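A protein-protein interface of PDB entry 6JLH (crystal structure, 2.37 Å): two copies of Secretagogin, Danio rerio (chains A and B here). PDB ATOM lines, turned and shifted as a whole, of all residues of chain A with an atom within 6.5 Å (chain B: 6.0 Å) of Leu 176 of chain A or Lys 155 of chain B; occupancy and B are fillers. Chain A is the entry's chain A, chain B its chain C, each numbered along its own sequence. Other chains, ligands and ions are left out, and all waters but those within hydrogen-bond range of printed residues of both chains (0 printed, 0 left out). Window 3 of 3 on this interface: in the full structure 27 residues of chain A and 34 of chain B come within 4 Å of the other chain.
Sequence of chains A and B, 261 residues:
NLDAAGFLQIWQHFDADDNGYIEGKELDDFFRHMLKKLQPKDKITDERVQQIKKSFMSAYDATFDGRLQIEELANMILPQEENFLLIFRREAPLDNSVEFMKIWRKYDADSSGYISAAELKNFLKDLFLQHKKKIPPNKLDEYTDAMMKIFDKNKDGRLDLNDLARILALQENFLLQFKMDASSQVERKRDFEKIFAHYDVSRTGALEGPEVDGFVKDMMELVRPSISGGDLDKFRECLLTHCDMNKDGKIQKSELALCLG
No position is printed for both chains.
Hydrophobic or aromatic side chains of chain A that line the printed part of chain B: Leu 176. Of the 11 printed residues of chain B, 5 touch a printed residue of chain A. Printed residues of chain B that touch a printed residue of chain A: Asp 18, Lys 153, Asn 154, Lys 155 and Asp 156. Among the printed residues, Asp or Glu carboxylates within 4 Å of a Lys or Arg side-chain nitrogen of the other chain: Lys 179 of chain A with Asp 18 of chain B.
Among the printed residues, pairs that only touch across the chains: Leu 176 of chain A with Lys 153 of chain B, Leu 176 of chain A with Asn 154 of chain B and Leu 222 of chain A with Asp 156 of chain B.
The side-chain amino group of Lys 179 of chain A lies within salt-bridge range of the side-chain carboxylate of Asp 18 of chain B, at 3.0 Å. The backbone carbonyl oxygen of Glu 221 of chain A lies close to the side-chain amide nitrogen of Asn 154 of chain B (3.3 Å). The backbone carbonyl oxygen (O) of Leu 222 of chain A is in hydrogen-bond range of the side-chain amide nitrogen (ND2) of Asn 154 of chain B (3.2 Å). O of Leu 176 of chain A is in hydrogen-bond range of NZ of Lys 155 of chain B (3.4 Å).
The side-chain carboxylate (OD1) of Asp 152 of chain B lies close to the backbone NH (N) of Lys 155 of chain B, 3.0 Å away.
Of the printed residues of chain B, Leu 222 of chain A touches Asn 154 (3.2 Å) and Asp 156 (3.97 Å). Of the printed residues of chain A, Lys 153 of chain B touches Leu 176 (3.7 Å). Of chain A, only Leu 176 comes within 4 Å of Lys 155 of chain B. The nearest printed residue of chain A that does not touch Lys 153 of chain B is Glu 221 of chain A (6.2 Å).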
ATOM      1  N   GLU A 172     -34.893 -15.429 -11.901  1.00  0.00           N
ATOM      2  CA  GLU A 172     -33.523 -14.931 -11.633  1.00  0.00           C
ATOM      3  C   GLU A 172     -33.157 -15.101 -10.144  1.00  0.00           C
ATOM      4  O   GLU A 172     -34.066 -15.241  -9.306  1.00  0.00           O
ATOM      5  CB  GLU A 172     -33.469 -13.470 -12.119  1.00  0.00           C
ATOM      6  CG  GLU A 172     -34.145 -12.450 -11.193  1.00  0.00           C
ATOM      7  CD  GLU A 172     -35.644 -12.224 -11.359  1.00  0.00           C
ATOM      8  OE1 GLU A 172     -36.250 -12.827 -12.282  1.00  0.00           O
ATOM      9  OE2 GLU A 172     -36.205 -11.448 -10.574  1.00  0.00           O
ATOM     10  N   ASN A 173     -31.851 -15.053  -9.881  1.00  0.00           N
ATOM     11  CA  ASN A 173     -31.194 -15.082  -8.553  1.00  0.00           C
ATOM     12  C   ASN A 173     -31.526 -13.801  -7.773  1.00  0.00           C
ATOM     13  O   ASN A 173     -30.976 -12.741  -8.078  1.00  0.00           O
ATOM     14  CB  ASN A 173     -29.684 -15.291  -8.691  1.00  0.00           C
ATOM     15  CG  ASN A 173     -28.966 -15.561  -7.375  1.00  0.00           C
ATOM     16  OD1 ASN A 173     -29.556 -15.459  -6.296  1.00  0.00           O
ATOM     17  ND2 ASN A 173     -27.698 -15.926  -7.441  1.00  0.00           N
ATOM     18  N   PHE A 174     -32.365 -13.948  -6.757  1.00  0.00           N
ATOM     19  CA  PHE A 174     -32.833 -12.925  -5.790  1.00  0.00           C
ATOM     20  C   PHE A 174     -31.673 -12.062  -5.287  1.00  0.00           C
ATOM     21  O   PHE A 174     -31.883 -10.835  -5.090  1.00  0.00           O
ATOM     22  CB  PHE A 174     -33.536 -13.648  -4.629  1.00  0.00           C
ATOM     23  CG  PHE A 174     -33.809 -12.791  -3.422  1.00  0.00           C
ATOM     24  CD1 PHE A 174     -34.955 -12.017  -3.362  1.00  0.00           C
ATOM     25  CD2 PHE A 174     -32.876 -12.691  -2.397  1.00  0.00           C
ATOM     26  CE1 PHE A 174     -35.170 -11.167  -2.291  1.00  0.00           C
ATOM     27  CE2 PHE A 174     -33.092 -11.859  -1.315  1.00  0.00           C
ATOM     28  CZ  PHE A 174     -34.246 -11.098  -1.277  1.00  0.00           C
ATOM     29  N   LEU A 175     -30.491 -12.649  -5.070  1.00  0.00           N
ATOM     30  CA  LEU A 175     -29.335 -11.942  -4.449  1.00  0.00           C
ATOM     31  C   LEU A 175     -28.656 -10.996  -5.449  1.00  0.00           C
ATOM     32  O   LEU A 175     -27.778 -10.233  -4.997  1.00  0.00           O
ATOM     33  CB  LEU A 175     -28.312 -12.949  -3.921  1.00  0.00           C
ATOM     34  CG  LEU A 175     -28.811 -13.929  -2.868  1.00  0.00           C
ATOM     35  CD1 LEU A 175     -27.695 -14.879  -2.456  1.00  0.00           C
ATOM     36  CD2 LEU A 175     -29.352 -13.188  -1.669  1.00  0.00           C
ATOM     37  N   LEU A 176     -29.006 -11.037  -6.740  1.00  0.00           N
ATOM     38  CA  LEU A 176     -28.305 -10.202  -7.752  1.00  0.00           C
ATOM     39  C   LEU A 176     -28.773  -8.747  -7.663  1.00  0.00           C
ATOM     40  O   LEU A 176     -28.086  -7.895  -8.196  1.00  0.00           O
ATOM     41  CB  LEU A 176     -28.502 -10.774  -9.161  1.00  0.00           C
ATOM     42  CG  LEU A 176     -27.795 -12.096  -9.441  1.00  0.00           C
ATOM     43  CD1 LEU A 176     -28.192 -12.633 -10.799  1.00  0.00           C
ATOM     44  CD2 LEU A 176     -26.285 -11.981  -9.348  1.00  0.00           C
ATOM     45  N   GLN A 177     -29.872  -8.478  -6.978  1.00  0.00           N
ATOM     46  CA  GLN A 177     -30.418  -7.108  -6.810  1.00  0.00           C
ATOM     47  C   GLN A 177     -29.574  -6.295  -5.818  1.00  0.00           C
ATOM     48  O   GLN A 177     -29.702  -5.059  -5.883  1.00  0.00           O
ATOM     49  CB  GLN A 177     -31.879  -7.164  -6.354  1.00  0.00           C
ATOM     50  CG  GLN A 177     -32.074  -7.720  -4.952  1.00  0.00           C
ATOM     51  CD  GLN A 177     -33.543  -7.892  -4.664  1.00  0.00           C
ATOM     52  OE1 GLN A 177     -34.215  -6.936  -4.305  1.00  0.00           O
ATOM     53  NE2 GLN A 177     -34.071  -9.099  -4.816  1.00  0.00           N
ATOM     54  N   PHE A 178     -28.766  -6.926  -4.941  1.00  0.00           N
ATOM     55  CA  PHE A 178     -28.015  -6.249  -3.845  1.00  0.00           C
ATOM     56  C   PHE A 178     -26.692  -5.687  -4.359  1.00  0.00           C
ATOM     57  O   PHE A 178     -26.081  -6.325  -5.203  1.00  0.00           O
ATOM     58  CB  PHE A 178     -27.788  -7.183  -2.658  1.00  0.00           C
ATOM     59  CG  PHE A 178     -29.095  -7.589  -2.049  1.00  0.00           C
ATOM     60  CD1 PHE A 178     -29.796  -6.713  -1.245  1.00  0.00           C
ATOM     61  CD2 PHE A 178     -29.655  -8.822  -2.346  1.00  0.00           C
ATOM     62  CE1 PHE A 178     -31.028  -7.073  -0.724  1.00  0.00           C
ATOM     63  CE2 PHE A 178     -30.883  -9.180  -1.830  1.00  0.00           C
ATOM     64  CZ  PHE A 178     -31.580  -8.298  -1.041  1.00  0.00           C
ATOM     65  N   LYS A 179     -26.277  -4.533  -3.822  1.00  0.00           N
ATOM     66  CA  LYS A 179     -25.213  -3.681  -4.412  1.00  0.00           C
ATOM     67  C   LYS A 179     -24.017  -3.595  -3.476  1.00  0.00           C
ATOM     68  O   LYS A 179     -24.194  -3.545  -2.266  1.00  0.00           O
ATOM     69  CB  LYS A 179     -25.788  -2.310  -4.778  1.00  0.00           C
ATOM     70  CG  LYS A 179     -26.163  -2.180  -6.245  1.00  0.00           C
ATOM     71  CD  LYS A 179     -25.047  -2.677  -7.192  1.00  0.00           C
ATOM     72  CE  LYS A 179     -24.809  -1.787  -8.398  1.00  0.00           C
ATOM     73  NZ  LYS A 179     -24.278  -0.448  -8.012  1.00  0.00           N
ATOM     74  N   GLU A 221     -24.154 -19.356  -6.841  1.00  0.00           N
ATOM     75  CA  GLU A 221     -24.325 -18.956  -8.232  1.00  0.00           C
ATOM     76  C   GLU A 221     -23.981 -17.466  -8.435  1.00  0.00           C
ATOM     77  O   GLU A 221     -24.002 -17.027  -9.568  1.00  0.00           O
ATOM     78  CB  GLU A 221     -25.720 -19.317  -8.747  1.00  0.00           C
ATOM     79  CG  GLU A 221     -25.883 -20.807  -8.932  1.00  0.00           C
ATOM     80  CD  GLU A 221     -27.256 -21.282  -9.398  1.00  0.00           C
ATOM     81  OE1 GLU A 221     -27.421 -22.499  -9.592  1.00  0.00           O
ATOM     82  OE2 GLU A 221     -28.147 -20.441  -9.610  1.00  0.00           O
ATOM     83  N   LEU A 222     -23.680 -16.722  -7.368  1.00  0.00           N
ATOM     84  CA  LEU A 222     -23.098 -15.358  -7.465  1.00  0.00           C
ATOM     85  C   LEU A 222     -21.706 -15.440  -8.083  1.00  0.00           C
ATOM     86  O   LEU A 222     -21.302 -14.418  -8.663  1.00  0.00           O
ATOM     87  CB  LEU A 222     -22.963 -14.694  -6.085  1.00  0.00           C
ATOM     88  CG  LEU A 222     -24.265 -14.358  -5.365  1.00  0.00           C
ATOM     89  CD1 LEU A 222     -23.962 -13.826  -3.984  1.00  0.00           C
ATOM     90  CD2 LEU A 222     -25.115 -13.365  -6.150  1.00  0.00           C
ATOM     91  N   ASP B  18     -31.314   0.317 -10.164  1.00  0.00           N
ATOM     92  CA  ASP B  18     -30.181  -0.622 -10.350  1.00  0.00           C
ATOM     93  C   ASP B  18     -30.571  -2.054  -9.920  1.00  0.00           C
ATOM     94  O   ASP B  18     -29.698  -2.769  -9.379  1.00  0.00           O
ATOM     95  CB  ASP B  18     -28.958  -0.093  -9.598  1.00  0.00           C
ATOM     96  CG  ASP B  18     -27.626  -0.466 -10.243  1.00  0.00           C
ATOM     97  OD1 ASP B  18     -27.605  -1.326 -11.164  1.00  0.00           O
ATOM     98  OD2 ASP B  18     -26.611   0.090  -9.819  1.00  0.00           O
ATOM     99  N   ASN B  19     -31.813  -2.493 -10.197  1.00  0.00           N
ATOM    100  CA  ASN B  19     -32.348  -3.823  -9.779  1.00  0.00           C
ATOM    101  C   ASN B  19     -32.281  -4.849 -10.927  1.00  0.00           C
ATOM    102  O   ASN B  19     -32.701  -5.982 -10.681  1.00  0.00           O
ATOM    103  CB  ASN B  19     -33.760  -3.690  -9.199  1.00  0.00           C
ATOM    104  CG  ASN B  19     -34.867  -3.687 -10.229  1.00  0.00           C
ATOM    105  OD1 ASN B  19     -34.726  -3.147 -11.320  1.00  0.00           O
ATOM    106  ND2 ASN B  19     -35.995  -4.273  -9.884  1.00  0.00           N
ATOM    107  N   GLY B  20     -31.787  -4.470 -12.120  1.00  0.00           N
ATOM    108  CA  GLY B  20     -31.567  -5.364 -13.278  1.00  0.00           C
ATOM    109  C   GLY B  20     -32.718  -5.388 -14.293  1.00  0.00           C
ATOM    110  O   GLY B  20     -32.652  -6.192 -15.254  1.00  0.00           O
ATOM    111  N   LYS B 149     -21.360  -6.269 -19.436  1.00  0.00           N
ATOM    112  CA  LYS B 149     -22.678  -6.144 -18.784  1.00  0.00           C
ATOM    113  C   LYS B 149     -23.624  -7.209 -19.352  1.00  0.00           C
ATOM    114  O   LYS B 149     -24.352  -7.797 -18.554  1.00  0.00           O
ATOM    115  CB  LYS B 149     -23.243  -4.735 -18.918  1.00  0.00           C
ATOM    116  CG  LYS B 149     -23.965  -4.250 -17.667  1.00  0.00           C
ATOM    117  CD  LYS B 149     -23.028  -3.872 -16.540  1.00  0.00           C
ATOM    118  CE  LYS B 149     -23.700  -3.008 -15.486  1.00  0.00           C
ATOM    119  NZ  LYS B 149     -24.971  -3.618 -15.031  1.00  0.00           N
ATOM    120  N   ASP B 152     -21.973 -11.093 -18.472  1.00  0.00           N
ATOM    121  CA  ASP B 152     -21.682 -11.354 -17.045  1.00  0.00           C
ATOM    122  C   ASP B 152     -23.010 -11.621 -16.321  1.00  0.00           C
ATOM    123  O   ASP B 152     -23.657 -10.671 -15.886  1.00  0.00           O
ATOM    124  CB  ASP B 152     -20.904 -10.188 -16.443  1.00  0.00           C
ATOM    125  CG  ASP B 152     -20.690 -10.391 -14.969  1.00  0.00           C
ATOM    126  OD1 ASP B 152     -21.045 -11.495 -14.505  1.00  0.00           O
ATOM    127  OD2 ASP B 152     -20.189  -9.455 -14.299  1.00  0.00           O
ATOM    128  N   LYS B 153     -23.400 -12.888 -16.199  1.00  0.00           N
ATOM    129  CA  LYS B 153     -24.771 -13.311 -15.787  1.00  0.00           C
ATOM    130  C   LYS B 153     -24.966 -13.114 -14.270  1.00  0.00           C
ATOM    131  O   LYS B 153     -26.090 -12.757 -13.873  1.00  0.00           O
ATOM    132  CB  LYS B 153     -25.015 -14.788 -16.153  1.00  0.00           C
ATOM    133  CG  LYS B 153     -25.101 -15.104 -17.643  1.00  0.00           C
ATOM    134  CD  LYS B 153     -25.937 -14.065 -18.406  1.00  0.00           C
ATOM    135  CE  LYS B 153     -26.385 -14.508 -19.789  1.00  0.00           C
ATOM    136  NZ  LYS B 153     -26.815 -13.353 -20.618  1.00  0.00           N
ATOM    137  N   ASN B 154     -23.928 -13.341 -13.458  1.00  0.00           N
ATOM    138  CA  ASN B 154     -24.012 -13.266 -11.980  1.00  0.00           C
ATOM    139  C   ASN B 154     -23.368 -11.961 -11.452  1.00  0.00           C
ATOM    140  O   ASN B 154     -23.245 -11.796 -10.210  1.00  0.00           O
ATOM    141  CB  ASN B 154     -23.458 -14.561 -11.380  1.00  0.00           C
ATOM    142  CG  ASN B 154     -22.027 -14.819 -11.791  1.00  0.00           C
ATOM    143  OD1 ASN B 154     -21.417 -13.970 -12.437  1.00  0.00           O
ATOM    144  ND2 ASN B 154     -21.509 -16.000 -11.472  1.00  0.00           N
ATOM    145  N   LYS B 155     -23.003 -11.039 -12.345  1.00  0.00           N
ATOM    146  CA  LYS B 155     -22.647  -9.626 -12.032  1.00  0.00           C
ATOM    147  C   LYS B 155     -21.433  -9.547 -11.103  1.00  0.00           C
ATOM    148  O   LYS B 155     -21.433  -8.696 -10.234  1.00  0.00           O
ATOM    149  CB  LYS B 155     -23.879  -8.921 -11.460  1.00  0.00           C
ATOM    150  CG  LYS B 155     -25.037  -8.835 -12.442  1.00  0.00           C
ATOM    151  CD  LYS B 155     -26.361  -8.510 -11.812  1.00  0.00           C
ATOM    152  CE  LYS B 155     -26.411  -7.140 -11.170  1.00  0.00           C
ATOM    153  NZ  LYS B 155     -27.761  -6.528 -11.320  1.00  0.00           N
ATOM    154  N   ASP B 156     -20.415 -10.390 -11.280  1.00  0.00           N
ATOM    155  CA  ASP B 156     -19.148 -10.289 -10.496  1.00  0.00           C
ATOM    156  C   ASP B 156     -18.084  -9.520 -11.286  1.00  0.00           C
ATOM    157  O   ASP B 156     -16.944  -9.508 -10.818  1.00  0.00           O
ATOM    158  CB  ASP B 156     -18.612 -11.661 -10.073  1.00  0.00           C
ATOM    159  CG  ASP B 156     -18.350 -12.643 -11.208  1.00  0.00           C
ATOM    160  OD1 ASP B 156     -18.459 -12.252 -12.367  1.00  0.00           O
ATOM    161  OD2 ASP B 156     -18.081 -13.822 -10.910  1.00  0.00           O
ATOM    162  N   GLY B 157     -18.421  -8.954 -12.455  1.00  0.00           N
ATOM    163  CA  GLY B 157     -17.491  -8.185 -13.308  1.00  0.00           C
ATOM    164  C   GLY B 157     -16.501  -9.093 -14.005  1.00  0.00           C
ATOM    165  O   GLY B 157     -15.448  -8.612 -14.444  1.00  0.00           O
ATOM    166  N   ARG B 158     -16.836 -10.374 -14.142  1.00  0.00           N
ATOM    167  CA  ARG B 158     -15.966 -11.364 -14.818  1.00  0.00           C
ATOM    168  C   ARG B 158     -16.799 -12.270 -15.710  1.00  0.00           C
ATOM    169  O   ARG B 158     -17.951 -12.533 -15.351  1.00  0.00           O
ATOM    170  CB  ARG B 158     -15.221 -12.188 -13.773  1.00  0.00           C
ATOM    171  CG  ARG B 158     -14.468 -11.320 -12.783  1.00  0.00           C
ATOM    172  CD  ARG B 158     -13.659 -12.144 -11.814  1.00  0.00           C
ATOM    173  NE  ARG B 158     -14.487 -12.916 -10.905  1.00  0.00           N
ATOM    174  CZ  ARG B 158     -14.072 -13.370  -9.717  1.00  0.00           C
ATOM    175  NH1 ARG B 158     -12.839 -13.130  -9.302  1.00  0.00           N
ATOM    176  NH2 ARG B 158     -14.882 -14.072  -8.942  1.00  0.00           N
